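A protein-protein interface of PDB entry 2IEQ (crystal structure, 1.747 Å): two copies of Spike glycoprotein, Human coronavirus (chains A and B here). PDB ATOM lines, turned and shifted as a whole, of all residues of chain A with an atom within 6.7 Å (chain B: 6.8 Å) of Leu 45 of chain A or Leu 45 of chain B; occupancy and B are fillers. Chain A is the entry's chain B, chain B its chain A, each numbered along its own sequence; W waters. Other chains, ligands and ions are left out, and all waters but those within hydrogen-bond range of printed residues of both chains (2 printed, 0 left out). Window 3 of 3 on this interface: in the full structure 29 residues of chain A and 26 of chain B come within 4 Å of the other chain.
The backbone carbonyl oxygen (O) of Leu 45 of chain B lies within hydrogen-bond range of the side-chain hydroxyl (OG1) of Thr 49 of chain B, 3.0 Å away.
OG1 of Thr 49 of chain A sits at hydrogen-bond distance from O of Leu 45 of chain A (3.2 Å).
The backbone carbonyl oxygen (O) of Asn 46 of chain A is in hydrogen-bond range of the side-chain hydroxyl (OG1) of Thr 49 of chain A (2.9 Å).
N of Leu 69 of chain A lies within hydrogen-bond range of OD1 of Asn 46 of chain A, 2.8 Å away.
Water W2 bridges OE1 of Gln 41 of chain A and OE1 of Gln 41 of chain B.
Water W1 lies within hydrogen-bond range of the side-chain amide oxygen (OE1) of Gln 41 of chain B (2.9 Å) and the side-chain amide oxygen (OE1) of Gln 41 of chain A (3.2 Å).
Gly 42 of chain A touches Gln 41 of chain B, but with the chains exchanged Gln 41 of chain A does not touch Gly 42 of chain B (7.6 Å).
Leu 45 of chain A touches Gln 41 of chain B, but with the chains exchanged Gln 41 of chain A does not touch Leu 45 of chain B (6.0 Å).
Leu 45 of chain B touches its own counterpart, Leu 45 of chain A.
Leu 48 of chain A touches its own counterpart, Leu 48 of chain B.
Positions printed for both chains: 40, 41, 42, 43, 44, 45, 46, 47, 48, 49, 50 and 69.
Gln 41 of chain A touches Gln 41 of chain B.
Gly 42 of chain A touches Gln 41 of chain B.
Gln 41 of chain B touches Leu 45 of chain A (CB to CD1, 3.9 Å).
CG of Leu 45 of chain B touches CD2 of Leu 45 of chain A, at 3.99 Å.
CD2 of Leu 48 of chain A touches CD2 of Leu 48 of chain B, at 3.5 Å.
Leu 48 of chain B touches Thr 49 of chain A.
Leu 69 of chain A touches Gln 40 of chain B (CB to OE1, 3.4 Å).
Leu 69 of chain A touches Ala 44 of chain B.
Hydrophobic or aromatic side chains of chain B within 4 Å of the printed part of chain A: Ala 44, Leu 45 and Leu 48.
Printed residues of chain A that touch a printed residue of chain B: Gln 41, Gly 42, Leu 45, Leu 48, Thr 49 and Leu 69.
Among the printed residues, no Asp or Glu carboxylate lies within 4 Å of a Lys or Arg side-chain nitrogen of the other chain.
Of the printed residues of chain B, Leu 45 of chain A touches Gln 41 (3.9 Å) and Leu 45 (3.99 Å).
Of the printed residues of chain B, Leu 48 of chain A touches Leu 48 (3.5 Å).
Of the printed residues of chain B, Leu 69 of chain A touches Gln 40 and Ala 44.
Gly 42 of chain B touches none of the printed residues of chain A.
Of the printed residues of chain A, Ala 44 of chain B touches Leu 69.
Of the printed residues of chain A, Leu 45 of chain B touches Leu 45 (3.99 Å).
Of the printed residues of chain A, Leu 48 of chain B touches Leu 48 (3.5 Å) and Thr 49 (3.7 Å).
The nearest printed residue of chain B that does not touch Leu 45 of chain A is Leu 48 of chain B (4.4 Å).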
ATOM      1  N   GLN A  40      -2.419   0.030  -2.830  1.00  0.00           N
ATOM      2  CA  GLN A  40      -1.549  -0.546  -1.777  1.00  0.00           C
ATOM      3  C   GLN A  40      -0.629  -1.617  -2.338  1.00  0.00           C
ATOM      4  O   GLN A  40       0.528  -1.679  -1.968  1.00  0.00           O
ATOM      5  CB  GLN A  40      -2.348  -1.139  -0.648  1.00  0.00           C
ATOM      6  CG  GLN A  40      -2.925  -0.136   0.320  1.00  0.00           C
ATOM      7  CD  GLN A  40      -3.649  -0.841   1.474  1.00  0.00           C
ATOM      8  OE1 GLN A  40      -3.241  -1.928   1.921  1.00  0.00           O
ATOM      9  NE2 GLN A  40      -4.713  -0.214   1.975  1.00  0.00           N
ATOM     10  N   GLN A  41      -1.147  -2.436  -3.262  1.00  0.00           N
ATOM     11  CA  GLN A  41      -0.358  -3.465  -3.908  1.00  0.00           C
ATOM     12  C   GLN A  41       0.680  -2.872  -4.870  1.00  0.00           C
ATOM     13  O   GLN A  41       1.822  -3.337  -4.918  1.00  0.00           O
ATOM     14  CB  GLN A  41      -1.258  -4.478  -4.609  1.00  0.00           C
ATOM     15  CG  GLN A  41      -2.018  -5.359  -3.624  1.00  0.00           C
ATOM     16  CD  GLN A  41      -2.985  -6.328  -4.268  1.00  0.00           C
ATOM     17  OE1 GLN A  41      -3.006  -6.499  -5.493  1.00  0.00           O
ATOM     18  NE2 GLN A  41      -3.786  -6.967  -3.442  1.00  0.00           N
ATOM     19  N   GLY A  42       0.298  -1.857  -5.632  1.00  0.00           N
ATOM     20  CA  GLY A  42       1.248  -1.160  -6.523  1.00  0.00           C
ATOM     21  C   GLY A  42       2.363  -0.484  -5.702  1.00  0.00           C
ATOM     22  O   GLY A  42       3.546  -0.583  -6.050  1.00  0.00           O
ATOM     23  N   SER A  43       1.997   0.219  -4.632  1.00  0.00           N
ATOM     24  CA  SER A  43       3.013   0.746  -3.694  1.00  0.00           C
ATOM     25  C   SER A  43       3.963  -0.340  -3.166  1.00  0.00           C
ATOM     26  O   SER A  43       5.195  -0.156  -3.240  1.00  0.00           O
ATOM     27  CB  SER A  43       2.365   1.479  -2.537  1.00  0.00           C
ATOM     28  OG  SER A  43       1.996   2.773  -2.959  1.00  0.00           O
ATOM     29  N   ALA A  44       3.412  -1.454  -2.658  1.00  0.00           N
ATOM     30  CA  ALA A  44       4.233  -2.575  -2.179  1.00  0.00           C
ATOM     31  C   ALA A  44       5.151  -3.108  -3.294  1.00  0.00           C
ATOM     32  O   ALA A  44       6.351  -3.365  -3.076  1.00  0.00           O
ATOM     33  CB  ALA A  44       3.408  -3.658  -1.594  1.00  0.00           C
ATOM     34  N   LEU A  45       4.591  -3.234  -4.491  1.00  0.00           N
ATOM     35  CA  LEU A  45       5.372  -3.626  -5.647  1.00  0.00           C
ATOM     36  C   LEU A  45       6.510  -2.679  -5.953  1.00  0.00           C
ATOM     37  O   LEU A  45       7.617  -3.135  -6.231  1.00  0.00           O
ATOM     38  CB  LEU A  45       4.484  -3.763  -6.869  1.00  0.00           C
ATOM     39  CG  LEU A  45       3.986  -5.192  -7.087  1.00  0.00           C
ATOM     40  CD1 LEU A  45       2.623  -5.213  -7.853  1.00  0.00           C
ATOM     41  CD2 LEU A  45       5.086  -5.996  -7.808  1.00  0.00           C
ATOM     42  N   ASN A  46       6.241  -1.370  -5.919  1.00  0.00           N
ATOM     43  CA  ASN A  46       7.263  -0.391  -6.264  1.00  0.00           C
ATOM     44  C   ASN A  46       8.399  -0.466  -5.245  1.00  0.00           C
ATOM     45  O   ASN A  46       9.580  -0.443  -5.613  1.00  0.00           O
ATOM     46  CB  ASN A  46       6.694   1.024  -6.340  1.00  0.00           C
ATOM     47  CG  ASN A  46       5.937   1.295  -7.642  1.00  0.00           C
ATOM     48  OD1 ASN A  46       6.102   0.585  -8.649  1.00  0.00           O
ATOM     49  ND2 ASN A  46       5.089   2.327  -7.625  1.00  0.00           N
ATOM     50  N   HIS A  47       8.026  -0.618  -3.979  1.00  0.00           N
ATOM     51  CA  HIS A  47       8.998  -0.626  -2.893  1.00  0.00           C
ATOM     52  C   HIS A  47       9.896  -1.841  -2.968  1.00  0.00           C
ATOM     53  O   HIS A  47      11.106  -1.741  -2.736  1.00  0.00           O
ATOM     54  CB  HIS A  47       8.309  -0.585  -1.528  1.00  0.00           C
ATOM     55  CG  HIS A  47       9.165   0.015  -0.454  1.00  0.00           C
ATOM     56  ND1 HIS A  47       9.848  -0.752   0.473  1.00  0.00           N
ATOM     57  CD2 HIS A  47       9.493   1.306  -0.192  1.00  0.00           C
ATOM     58  CE1 HIS A  47      10.534   0.043   1.275  1.00  0.00           C
ATOM     59  NE2 HIS A  47      10.336   1.295   0.893  1.00  0.00           N
ATOM     60  N   LEU A  48       9.290  -2.984  -3.271  1.00  0.00           N
ATOM     61  CA  LEU A  48      10.000  -4.251  -3.393  1.00  0.00           C
ATOM     62  C   LEU A  48      11.018  -4.200  -4.527  1.00  0.00           C
ATOM     63  O   LEU A  48      12.182  -4.566  -4.346  1.00  0.00           O
ATOM     64  CB  LEU A  48       9.014  -5.393  -3.626  1.00  0.00           C
ATOM     65  CG  LEU A  48       9.519  -6.834  -3.730  1.00  0.00           C
ATOM     66  CD1 LEU A  48       9.936  -7.404  -2.365  1.00  0.00           C
ATOM     67  CD2 LEU A  48       8.445  -7.696  -4.344  1.00  0.00           C
ATOM     68  N   THR A  49      10.571  -3.749  -5.692  1.00  0.00           N
ATOM     69  CA  THR A  49      11.420  -3.745  -6.864  1.00  0.00           C
ATOM     70  C   THR A  49      12.565  -2.760  -6.680  1.00  0.00           C
ATOM     71  O   THR A  49      13.701  -3.052  -7.069  1.00  0.00           O
ATOM     72  CB  THR A  49      10.648  -3.405  -8.132  1.00  0.00           C
ATOM     73  OG1 THR A  49      10.045  -2.122  -7.972  1.00  0.00           O
ATOM     74  CG2 THR A  49       9.564  -4.440  -8.383  1.00  0.00           C
ATOM     75  N   SER A  50      12.280  -1.603  -6.083  1.00  0.00           N
ATOM     76  CA  SER A  50      13.337  -0.628  -5.872  1.00  0.00           C
ATOM     77  C   SER A  50      14.316  -1.060  -4.781  1.00  0.00           C
ATOM     78  O   SER A  50      15.522  -0.869  -4.948  1.00  0.00           O
ATOM     79  CB  SER A  50      12.812   0.789  -5.684  1.00  0.00           C
ATOM     80  OG  SER A  50      13.519   1.654  -6.576  1.00  0.00           O
ATOM     81  N   LEU A  69       5.194   1.853 -10.996  1.00  0.00           N
ATOM     82  CA  LEU A  69       3.904   1.516 -11.591  1.00  0.00           C
ATOM     83  C   LEU A  69       2.910   2.699 -11.533  1.00  0.00           C
ATOM     84  O   LEU A  69       3.076   3.658 -10.734  1.00  0.00           O
ATOM     85  CB  LEU A  69       3.307   0.296 -10.891  1.00  0.00           C
ATOM     86  CG  LEU A  69       4.105  -1.009 -10.887  1.00  0.00           C
ATOM     87  CD1 LEU A  69       3.911  -1.705  -9.559  1.00  0.00           C
ATOM     88  CD2 LEU A  69       3.703  -1.917 -12.042  1.00  0.00           C
ATOM     89  N   GLN B  40      -1.402  -4.326 -15.546  1.00  0.00           N
ATOM     90  CA  GLN B  40      -0.013  -3.823 -15.408  1.00  0.00           C
ATOM     91  C   GLN B  40       0.692  -4.429 -14.194  1.00  0.00           C
ATOM     92  O   GLN B  40       1.859  -4.849 -14.270  1.00  0.00           O
ATOM     93  CB  GLN B  40       0.020  -2.320 -15.308  1.00  0.00           C
ATOM     94  CG  GLN B  40       1.414  -1.807 -15.023  1.00  0.00           C
ATOM     95  CD  GLN B  40       1.436  -0.326 -14.857  1.00  0.00           C
ATOM     96  OE1 GLN B  40       1.517   0.168 -13.743  1.00  0.00           O
ATOM     97  NE2 GLN B  40       1.318   0.403 -15.964  1.00  0.00           N
ATOM     98  N   GLN B  41       0.008  -4.497 -13.053  1.00  0.00           N
ATOM     99  CA  GLN B  41       0.636  -5.068 -11.863  1.00  0.00           C
ATOM    100  C   GLN B  41       0.858  -6.572 -11.940  1.00  0.00           C
ATOM    101  O   GLN B  41       1.878  -7.067 -11.459  1.00  0.00           O
ATOM    102  CB  GLN B  41      -0.174  -4.770 -10.605  1.00  0.00           C
ATOM    103  CG  GLN B  41      -0.170  -3.298 -10.314  1.00  0.00           C
ATOM    104  CD  GLN B  41      -0.979  -2.917  -9.089  1.00  0.00           C
ATOM    105  OE1 GLN B  41      -1.431  -3.776  -8.344  1.00  0.00           O
ATOM    106  NE2 GLN B  41      -1.152  -1.614  -8.881  1.00  0.00           N
ATOM    107  N   GLY B  42      -0.103  -7.305 -12.495  1.00  0.00           N
ATOM    108  CA  GLY B  42       0.051  -8.733 -12.703  1.00  0.00           C
ATOM    109  C   GLY B  42       1.277  -9.011 -13.566  1.00  0.00           C
ATOM    110  O   GLY B  42       2.001  -9.970 -13.303  1.00  0.00           O
ATOM    111  N   SER B  43       1.499  -8.162 -14.576  1.00  0.00           N
ATOM    112  CA  SER B  43       2.628  -8.323 -15.513  1.00  0.00           C
ATOM    113  C   SER B  43       3.944  -8.068 -14.785  1.00  0.00           C
ATOM    114  O   SER B  43       4.897  -8.843 -14.924  1.00  0.00           O
ATOM    115  CB  SER B  43       2.503  -7.376 -16.706  1.00  0.00           C
ATOM    116  OG  SER B  43       1.609  -7.927 -17.679  1.00  0.00           O
ATOM    117  N   ALA B  44       3.971  -7.008 -13.978  1.00  0.00           N
ATOM    118  CA  ALA B  44       5.146  -6.696 -13.173  1.00  0.00           C
ATOM    119  C   ALA B  44       5.463  -7.831 -12.200  1.00  0.00           C
ATOM    120  O   ALA B  44       6.632  -8.232 -12.083  1.00  0.00           O
ATOM    121  CB  ALA B  44       4.976  -5.380 -12.461  1.00  0.00           C
ATOM    122  N   LEU B  45       4.439  -8.380 -11.537  1.00  0.00           N
ATOM    123  CA  LEU B  45       4.616  -9.537 -10.659  1.00  0.00           C
ATOM    124  C   LEU B  45       5.112 -10.759 -11.407  1.00  0.00           C
ATOM    125  O   LEU B  45       5.910 -11.521 -10.850  1.00  0.00           O
ATOM    126  CB  LEU B  45       3.334  -9.941  -9.930  1.00  0.00           C
ATOM    127  CG  LEU B  45       3.076  -9.363  -8.555  1.00  0.00           C
ATOM    128  CD1 LEU B  45       1.561  -9.302  -8.282  1.00  0.00           C
ATOM    129  CD2 LEU B  45       3.808 -10.219  -7.516  1.00  0.00           C
ATOM    130  N   ASN B  46       4.610 -10.979 -12.626  1.00  0.00           N
ATOM    131  CA  ASN B  46       5.052 -12.143 -13.410  1.00  0.00           C
ATOM    132  C   ASN B  46       6.548 -12.068 -13.636  1.00  0.00           C
ATOM    133  O   ASN B  46       7.288 -12.978 -13.226  1.00  0.00           O
ATOM    134  CB  ASN B  46       4.315 -12.269 -14.744  1.00  0.00           C
ATOM    135  CG  ASN B  46       2.938 -12.883 -14.590  1.00  0.00           C
ATOM    136  OD1 ASN B  46       2.107 -12.827 -15.511  1.00  0.00           O
ATOM    137  ND2 ASN B  46       2.691 -13.497 -13.429  1.00  0.00           N
ATOM    138  N   HIS B  47       6.970 -10.959 -14.245  1.00  0.00           N
ATOM    139  CA  HIS B  47       8.367 -10.670 -14.508  1.00  0.00           C
ATOM    140  C   HIS B  47       9.243 -10.905 -13.277  1.00  0.00           C
ATOM    141  O   HIS B  47      10.245 -11.629 -13.340  1.00  0.00           O
ATOM    142  CB  HIS B  47       8.515  -9.231 -14.997  1.00  0.00           C
ATOM    143  CG  HIS B  47       9.849  -8.940 -15.615  1.00  0.00           C
ATOM    144  ND1 HIS B  47      10.984  -8.699 -14.865  1.00  0.00           N
ATOM    145  CD2 HIS B  47      10.230  -8.859 -16.916  1.00  0.00           C
ATOM    146  CE1 HIS B  47      12.003  -8.479 -15.680  1.00  0.00           C
ATOM    147  NE2 HIS B  47      11.574  -8.574 -16.927  1.00  0.00           N
ATOM    148  N   LEU B  48       8.843 -10.308 -12.159  1.00  0.00           N
ATOM    149  CA  LEU B  48       9.587 -10.367 -10.909  1.00  0.00           C
ATOM    150  C   LEU B  48       9.657 -11.776 -10.317  1.00  0.00           C
ATOM    151  O   LEU B  48      10.611 -12.108  -9.606  1.00  0.00           O
ATOM    152  CB  LEU B  48       8.950  -9.418  -9.903  1.00  0.00           C
ATOM    153  CG  LEU B  48       9.787  -8.866  -8.766  1.00  0.00           C
ATOM    154  CD1 LEU B  48      10.768  -7.858  -9.302  1.00  0.00           C
ATOM    155  CD2 LEU B  48       8.871  -8.209  -7.764  1.00  0.00           C
ATOM    156  N   THR B  49       8.652 -12.605 -10.588  1.00  0.00           N
ATOM    157  CA  THR B  49       8.717 -13.979 -10.125  1.00  0.00           C
ATOM    158  C   THR B  49       9.641 -14.764 -11.058  1.00  0.00           C
ATOM    159  O   THR B  49      10.451 -15.566 -10.607  1.00  0.00           O
ATOM    160  CB  THR B  49       7.325 -14.624  -9.995  1.00  0.00           C
ATOM    161  OG1 THR B  49       6.517 -13.834  -9.110  1.00  0.00           O
ATOM    162  CG2 THR B  49       7.430 -16.049  -9.434  1.00  0.00           C
ATOM    163  N   SER B  50       9.535 -14.483 -12.351  1.00  0.00           N
ATOM    164  CA  SER B  50      10.389 -15.069 -13.380  1.00  0.00           C
ATOM    165  C   SER B  50      11.889 -14.726 -13.235  1.00  0.00           C
ATOM    166  O   SER B  50      12.712 -15.168 -14.055  1.00  0.00           O
ATOM    167  CB  SER B  50       9.878 -14.632 -14.760  1.00  0.00           C
ATOM    168  OG  SER B  50      10.903 -14.002 -15.518  1.00  0.00           O
ATOM    169  N   LEU B  69       0.113 -15.763 -13.267  1.00  0.00           N
ATOM    170  CA  LEU B  69      -1.012 -14.980 -12.751  1.00  0.00           C
ATOM    171  C   LEU B  69      -2.085 -14.754 -13.807  1.00  0.00           C
ATOM    172  O   LEU B  69      -1.787 -14.449 -14.959  1.00  0.00           O
ATOM    173  CB  LEU B  69      -0.540 -13.629 -12.187  1.00  0.00           C
ATOM    174  CG  LEU B  69      -0.193 -13.499 -10.693  1.00  0.00           C
ATOM    175  CD1 LEU B  69       0.423 -14.758 -10.133  1.00  0.00           C
ATOM    176  CD2 LEU B  69       0.747 -12.344 -10.472  1.00  0.00           C
HETATM  177  O   HOH W   1      -3.948  -5.302  -8.334  1.00  0.00           O
HETATM  178  O   HOH W   2      -1.162  -6.550  -7.343  1.00  0.00           O
